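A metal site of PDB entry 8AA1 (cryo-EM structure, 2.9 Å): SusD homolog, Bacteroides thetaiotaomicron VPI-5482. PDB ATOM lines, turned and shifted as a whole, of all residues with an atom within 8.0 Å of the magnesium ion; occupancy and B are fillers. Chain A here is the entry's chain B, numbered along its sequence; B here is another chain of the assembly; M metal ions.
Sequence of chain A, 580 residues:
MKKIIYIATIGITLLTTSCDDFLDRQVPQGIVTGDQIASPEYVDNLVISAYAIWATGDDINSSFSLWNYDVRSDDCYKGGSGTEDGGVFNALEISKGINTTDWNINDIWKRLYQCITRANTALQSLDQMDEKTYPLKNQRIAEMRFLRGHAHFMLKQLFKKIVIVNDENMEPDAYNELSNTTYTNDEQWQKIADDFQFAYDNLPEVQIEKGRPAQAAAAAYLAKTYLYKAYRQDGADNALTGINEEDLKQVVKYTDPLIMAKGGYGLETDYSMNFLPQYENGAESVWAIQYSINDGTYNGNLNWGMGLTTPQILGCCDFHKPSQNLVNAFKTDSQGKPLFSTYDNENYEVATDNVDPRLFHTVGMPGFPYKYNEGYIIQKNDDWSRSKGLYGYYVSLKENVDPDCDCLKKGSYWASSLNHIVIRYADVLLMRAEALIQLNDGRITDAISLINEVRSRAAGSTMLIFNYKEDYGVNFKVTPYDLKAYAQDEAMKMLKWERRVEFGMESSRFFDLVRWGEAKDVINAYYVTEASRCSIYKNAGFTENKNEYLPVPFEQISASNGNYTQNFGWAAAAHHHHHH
The side-chain amide oxygen (OD1) of Asn 419 is bound to the magnesium ion (2.1 Å). The side-chain amide nitrogen (ND2) of Asn 689 of chain B is bound to the magnesium ion (2.1 Å). O of Tyr 291 is bound to the magnesium ion (2.1 Å). The magnesium ion is bound by OE1 of Glu 280, at 2.5 Å. The magnesium ion has four donor atoms within binding distance. Slightly farther from the magnesium ion lies the backbone carbonyl oxygen (O) of Ser 417 (2.6 Å).
O of Ser 417 lies close to ND2 of Asn 689 of chain B, at 3.3 Å. ND2 of Asn 419 sits at hydrogen-bond distance from OD1 of Asn 281 (3.2 Å). ND2 of Asn 419 is in hydrogen-bond range of OE1 of Gln 290 (2.6 Å). N of Ser 417 lies within hydrogen-bond range of O of Cys 407, 3.3 Å away. OD1 of Asn 419 lies close to O of Ser 417 (3.3 Å). The side-chain carboxylate (OD2) of Asp 684 of chain B is in hydrogen-bond range of the backbone NH (N) of Asn 689 of chain B (2.7 Å).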
ATOM      1  N   PRO A 277     -16.612   7.452 -21.652  1.00  0.00           N
ATOM      2  CA  PRO A 277     -17.026   6.063 -21.376  1.00  0.00           C
ATOM      3  C   PRO A 277     -18.060   5.533 -22.345  1.00  0.00           C
ATOM      4  O   PRO A 277     -18.074   4.325 -22.620  1.00  0.00           O
ATOM      5  CB  PRO A 277     -17.582   6.148 -19.944  1.00  0.00           C
ATOM      6  CG  PRO A 277     -16.986   7.388 -19.364  1.00  0.00           C
ATOM      7  CD  PRO A 277     -16.853   8.347 -20.508  1.00  0.00           C
ATOM      8  N   GLU A 280     -16.341   3.778 -25.680  1.00  0.00           N
ATOM      9  CA  GLU A 280     -15.198   2.902 -25.513  1.00  0.00           C
ATOM     10  C   GLU A 280     -15.101   1.917 -26.673  1.00  0.00           C
ATOM     11  O   GLU A 280     -16.113   1.559 -27.299  1.00  0.00           O
ATOM     12  CB  GLU A 280     -15.286   2.138 -24.191  1.00  0.00           C
ATOM     13  CG  GLU A 280     -15.084   3.008 -22.957  1.00  0.00           C
ATOM     14  CD  GLU A 280     -14.979   2.193 -21.685  1.00  0.00           C
ATOM     15  OE1 GLU A 280     -14.907   0.954 -21.781  1.00  0.00           O
ATOM     16  OE2 GLU A 280     -14.990   2.799 -20.595  1.00  0.00           O
ATOM     17  N   ASN A 281     -13.874   1.478 -26.950  1.00  0.00           N
ATOM     18  CA  ASN A 281     -13.599   0.524 -28.029  1.00  0.00           C
ATOM     19  C   ASN A 281     -14.114   1.031 -29.370  1.00  0.00           C
ATOM     20  O   ASN A 281     -14.764   0.319 -30.136  1.00  0.00           O
ATOM     21  CB  ASN A 281     -14.179  -0.859 -27.708  1.00  0.00           C
ATOM     22  CG  ASN A 281     -13.597  -1.459 -26.449  1.00  0.00           C
ATOM     23  OD1 ASN A 281     -12.438  -1.206 -26.112  1.00  0.00           O
ATOM     24  ND2 ASN A 281     -14.384  -2.265 -25.746  1.00  0.00           N
ATOM     25  N   ALA A 288      -6.556  -0.871 -26.472  1.00  0.00           N
ATOM     26  CA  ALA A 288      -6.707  -0.190 -25.211  1.00  0.00           C
ATOM     27  C   ALA A 288      -6.747  -1.207 -24.072  1.00  0.00           C
ATOM     28  O   ALA A 288      -7.088  -2.376 -24.279  1.00  0.00           O
ATOM     29  CB  ALA A 288      -7.983   0.671 -25.181  1.00  0.00           C
ATOM     30  N   ILE A 289      -6.387  -0.742 -22.882  1.00  0.00           N
ATOM     31  CA  ILE A 289      -6.484  -1.566 -21.686  1.00  0.00           C
ATOM     32  C   ILE A 289      -7.924  -1.538 -21.204  1.00  0.00           C
ATOM     33  O   ILE A 289      -8.491  -0.465 -20.977  1.00  0.00           O
ATOM     34  CB  ILE A 289      -5.526  -1.068 -20.589  1.00  0.00           C
ATOM     35  CG1 ILE A 289      -4.090  -1.029 -21.119  1.00  0.00           C
ATOM     36  CG2 ILE A 289      -5.618  -1.962 -19.359  1.00  0.00           C
ATOM     37  CD1 ILE A 289      -3.581  -2.372 -21.588  1.00  0.00           C
ATOM     38  N   GLN A 290      -8.522  -2.711 -21.053  1.00  0.00           N
ATOM     39  CA  GLN A 290      -9.934  -2.825 -20.721  1.00  0.00           C
ATOM     40  C   GLN A 290     -10.116  -2.707 -19.211  1.00  0.00           C
ATOM     41  O   GLN A 290      -9.787  -3.634 -18.465  1.00  0.00           O
ATOM     42  CB  GLN A 290     -10.509  -4.141 -21.240  1.00  0.00           C
ATOM     43  CG  GLN A 290     -10.294  -4.354 -22.734  1.00  0.00           C
ATOM     44  CD  GLN A 290     -11.019  -3.327 -23.581  1.00  0.00           C
ATOM     45  OE1 GLN A 290     -12.079  -2.818 -23.192  1.00  0.00           O
ATOM     46  NE2 GLN A 290     -10.457  -3.014 -24.733  1.00  0.00           N
ATOM     47  N   TYR A 291     -10.650  -1.577 -18.764  1.00  0.00           N
ATOM     48  CA  TYR A 291     -10.989  -1.368 -17.365  1.00  0.00           C
ATOM     49  C   TYR A 291     -12.484  -1.554 -17.191  1.00  0.00           C
ATOM     50  O   TYR A 291     -13.280  -1.016 -17.972  1.00  0.00           O
ATOM     51  CB  TYR A 291     -10.567   0.031 -16.894  1.00  0.00           C
ATOM     52  CG  TYR A 291      -9.068   0.226 -16.862  1.00  0.00           C
ATOM     53  CD1 TYR A 291      -8.300  -0.327 -15.844  1.00  0.00           C
ATOM     54  CD2 TYR A 291      -8.419   0.977 -17.826  1.00  0.00           C
ATOM     55  CE1 TYR A 291      -6.938  -0.157 -15.799  1.00  0.00           C
ATOM     56  CE2 TYR A 291      -7.050   1.157 -17.790  1.00  0.00           C
ATOM     57  CZ  TYR A 291      -6.311   0.592 -16.781  1.00  0.00           C
ATOM     58  OH  TYR A 291      -4.953   0.770 -16.731  1.00  0.00           O
ATOM     59  N   SER A 292     -12.871  -2.317 -16.164  1.00  0.00           N
ATOM     60  CA  SER A 292     -14.254  -2.712 -15.967  1.00  0.00           C
ATOM     61  C   SER A 292     -14.682  -2.411 -14.548  1.00  0.00           C
ATOM     62  O   SER A 292     -13.874  -2.305 -13.624  1.00  0.00           O
ATOM     63  CB  SER A 292     -14.447  -4.208 -16.270  1.00  0.00           C
ATOM     64  OG  SER A 292     -13.606  -4.999 -15.458  1.00  0.00           O
ATOM     65  N   ILE A 293     -16.002  -2.265 -14.381  1.00  0.00           N
ATOM     66  CA  ILE A 293     -16.612  -2.027 -13.079  1.00  0.00           C
ATOM     67  C   ILE A 293     -17.758  -3.020 -12.899  1.00  0.00           C
ATOM     68  O   ILE A 293     -18.341  -3.507 -13.884  1.00  0.00           O
ATOM     69  CB  ILE A 293     -17.104  -0.570 -12.934  1.00  0.00           C
ATOM     70  CG1 ILE A 293     -17.369  -0.231 -11.461  1.00  0.00           C
ATOM     71  CG2 ILE A 293     -18.348  -0.333 -13.771  1.00  0.00           C
ATOM     72  CD1 ILE A 293     -17.860   1.184 -11.245  1.00  0.00           C
ATOM     73  N   ASN A 301     -11.981  -3.582 -11.734  1.00  0.00           N
ATOM     74  CA  ASN A 301     -10.700  -3.377 -12.408  1.00  0.00           C
ATOM     75  C   ASN A 301     -10.648  -1.959 -12.962  1.00  0.00           C
ATOM     76  O   ASN A 301     -10.624  -1.718 -14.178  1.00  0.00           O
ATOM     77  CB  ASN A 301     -10.488  -4.421 -13.489  1.00  0.00           C
ATOM     78  CG  ASN A 301     -10.217  -5.794 -12.931  1.00  0.00           C
ATOM     79  OD1 ASN A 301      -9.667  -5.942 -11.842  1.00  0.00           O
ATOM     80  ND2 ASN A 301     -10.600  -6.822 -13.672  1.00  0.00           N
ATOM     81  N   LEU A 302     -10.635  -0.998 -12.043  1.00  0.00           N
ATOM     82  CA  LEU A 302     -10.614   0.409 -12.413  1.00  0.00           C
ATOM     83  C   LEU A 302      -9.191   0.857 -12.721  1.00  0.00           C
ATOM     84  O   LEU A 302      -8.212   0.158 -12.443  1.00  0.00           O
ATOM     85  CB  LEU A 302     -11.215   1.264 -11.296  1.00  0.00           C
ATOM     86  CG  LEU A 302     -12.622   0.864 -10.836  1.00  0.00           C
ATOM     87  CD1 LEU A 302     -13.057   1.733  -9.665  1.00  0.00           C
ATOM     88  CD2 LEU A 302     -13.608   0.985 -11.984  1.00  0.00           C
ATOM     89  N   CYS A 407     -19.809   5.380 -13.712  1.00  0.00           N
ATOM     90  CA  CYS A 407     -18.632   4.575 -13.996  1.00  0.00           C
ATOM     91  C   CYS A 407     -17.465   4.920 -13.089  1.00  0.00           C
ATOM     92  O   CYS A 407     -16.375   4.357 -13.251  1.00  0.00           O
ATOM     93  CB  CYS A 407     -18.237   4.743 -15.464  1.00  0.00           C
ATOM     94  SG  CYS A 407     -17.518   6.366 -15.847  1.00  0.00           S
ATOM     95  N   SER A 416     -11.978   5.351 -12.436  1.00  0.00           N
ATOM     96  CA  SER A 416     -13.074   5.063 -13.346  1.00  0.00           C
ATOM     97  C   SER A 416     -12.749   3.843 -14.198  1.00  0.00           C
ATOM     98  O   SER A 416     -11.636   3.295 -14.145  1.00  0.00           O
ATOM     99  CB  SER A 416     -13.379   6.267 -14.244  1.00  0.00           C
ATOM    100  OG  SER A 416     -12.249   6.612 -15.019  1.00  0.00           O
ATOM    101  N   SER A 417     -13.731   3.418 -14.986  1.00  0.00           N
ATOM    102  CA  SER A 417     -13.593   2.280 -15.876  1.00  0.00           C
ATOM    103  C   SER A 417     -13.259   2.688 -17.299  1.00  0.00           C
ATOM    104  O   SER A 417     -13.312   1.853 -18.206  1.00  0.00           O
ATOM    105  CB  SER A 417     -14.867   1.428 -15.858  1.00  0.00           C
ATOM    106  OG  SER A 417     -15.979   2.198 -16.295  1.00  0.00           O
ATOM    107  N   LEU A 418     -12.924   3.955 -17.519  1.00  0.00           N
ATOM    108  CA  LEU A 418     -12.570   4.425 -18.852  1.00  0.00           C
ATOM    109  C   LEU A 418     -11.310   3.719 -19.348  1.00  0.00           C
ATOM    110  O   LEU A 418     -10.320   3.620 -18.620  1.00  0.00           O
ATOM    111  CB  LEU A 418     -12.362   5.940 -18.848  1.00  0.00           C
ATOM    112  CG  LEU A 418     -12.028   6.584 -20.186  1.00  0.00           C
ATOM    113  CD1 LEU A 418     -13.141   6.346 -21.193  1.00  0.00           C
ATOM    114  CD2 LEU A 418     -11.788   8.079 -20.008  1.00  0.00           C
ATOM    115  N   ASN A 419     -11.364   3.228 -20.583  1.00  0.00           N
ATOM    116  CA  ASN A 419     -10.237   2.492 -21.138  1.00  0.00           C
ATOM    117  C   ASN A 419      -9.078   3.427 -21.450  1.00  0.00           C
ATOM    118  O   ASN A 419      -9.264   4.557 -21.893  1.00  0.00           O
ATOM    119  CB  ASN A 419     -10.667   1.753 -22.401  1.00  0.00           C
ATOM    120  CG  ASN A 419     -11.671   0.655 -22.125  1.00  0.00           C
ATOM    121  OD1 ASN A 419     -12.203   0.548 -21.022  1.00  0.00           O
ATOM    122  ND2 ASN A 419     -11.934  -0.177 -23.134  1.00  0.00           N
ATOM    123  N   HIS A 420      -7.864   2.940 -21.204  1.00  0.00           N
ATOM    124  CA  HIS A 420      -6.639   3.666 -21.537  1.00  0.00           C
ATOM    125  C   HIS A 420      -6.196   3.222 -22.923  1.00  0.00           C
ATOM    126  O   HIS A 420      -5.724   2.091 -23.107  1.00  0.00           O
ATOM    127  CB  HIS A 420      -5.549   3.412 -20.499  1.00  0.00           C
ATOM    128  CG  HIS A 420      -4.185   3.786 -20.960  1.00  0.00           C
ATOM    129  ND1 HIS A 420      -3.849   5.073 -21.341  1.00  0.00           N
ATOM    130  CD2 HIS A 420      -3.062   3.049 -21.108  1.00  0.00           C
ATOM    131  CE1 HIS A 420      -2.574   5.106 -21.697  1.00  0.00           C
ATOM    132  NE2 HIS A 420      -2.078   3.890 -21.565  1.00  0.00           N
ATOM    133  N   ASP B 684     -11.341  -7.962 -18.409  1.00  0.00           N
ATOM    134  CA  ASP B 684     -12.515  -7.865 -19.272  1.00  0.00           C
ATOM    135  C   ASP B 684     -12.040  -8.029 -20.719  1.00  0.00           C
ATOM    136  O   ASP B 684     -11.887  -7.072 -21.474  1.00  0.00           O
ATOM    137  CB  ASP B 684     -13.235  -6.534 -19.058  1.00  0.00           C
ATOM    138  CG  ASP B 684     -14.558  -6.460 -19.791  1.00  0.00           C
ATOM    139  OD1 ASP B 684     -15.015  -7.505 -20.295  1.00  0.00           O
ATOM    140  OD2 ASP B 684     -15.139  -5.358 -19.863  1.00  0.00           O
ATOM    141  N   GLY B 687     -14.531  -6.666 -23.342  1.00  0.00           N
ATOM    142  CA  GLY B 687     -14.625  -5.228 -23.443  1.00  0.00           C
ATOM    143  C   GLY B 687     -16.037  -4.710 -23.264  1.00  0.00           C
ATOM    144  O   GLY B 687     -16.518  -3.898 -24.058  1.00  0.00           O
ATOM    145  N   SER B 688     -16.710  -5.165 -22.205  1.00  0.00           N
ATOM    146  CA  SER B 688     -18.087  -4.769 -21.920  1.00  0.00           C
ATOM    147  C   SER B 688     -18.203  -3.990 -20.612  1.00  0.00           C
ATOM    148  O   SER B 688     -19.316  -3.848 -20.082  1.00  0.00           O
ATOM    149  CB  SER B 688     -19.003  -5.991 -21.892  1.00  0.00           C
ATOM    150  OG  SER B 688     -18.586  -6.913 -20.895  1.00  0.00           O
ATOM    151  N   ASN B 689     -17.092  -3.484 -20.091  1.00  0.00           N
ATOM    152  CA  ASN B 689     -17.065  -2.750 -18.829  1.00  0.00           C
ATOM    153  C   ASN B 689     -17.671  -3.577 -17.696  1.00  0.00           C
ATOM    154  O   ASN B 689     -18.405  -3.061 -16.845  1.00  0.00           O
ATOM    155  CB  ASN B 689     -17.781  -1.399 -18.945  1.00  0.00           C
ATOM    156  CG  ASN B 689     -16.990  -0.400 -19.766  1.00  0.00           C
ATOM    157  OD1 ASN B 689     -17.445   0.058 -20.817  1.00  0.00           O
ATOM    158  ND2 ASN B 689     -15.801  -0.044 -19.288  1.00  0.00           N
ATOM    159  N   GLY B 690     -17.354  -4.860 -17.672  1.00  0.00           N
ATOM    160  CA  GLY B 690     -17.841  -5.730 -16.612  1.00  0.00           C
ATOM    161  C   GLY B 690     -19.301  -6.106 -16.804  1.00  0.00           C
ATOM    162  O   GLY B 690     -19.800  -6.239 -17.921  1.00  0.00           O
HETATM  163 MG    MG M   1     -13.759  -0.125 -19.847  1.00  0.00          MG
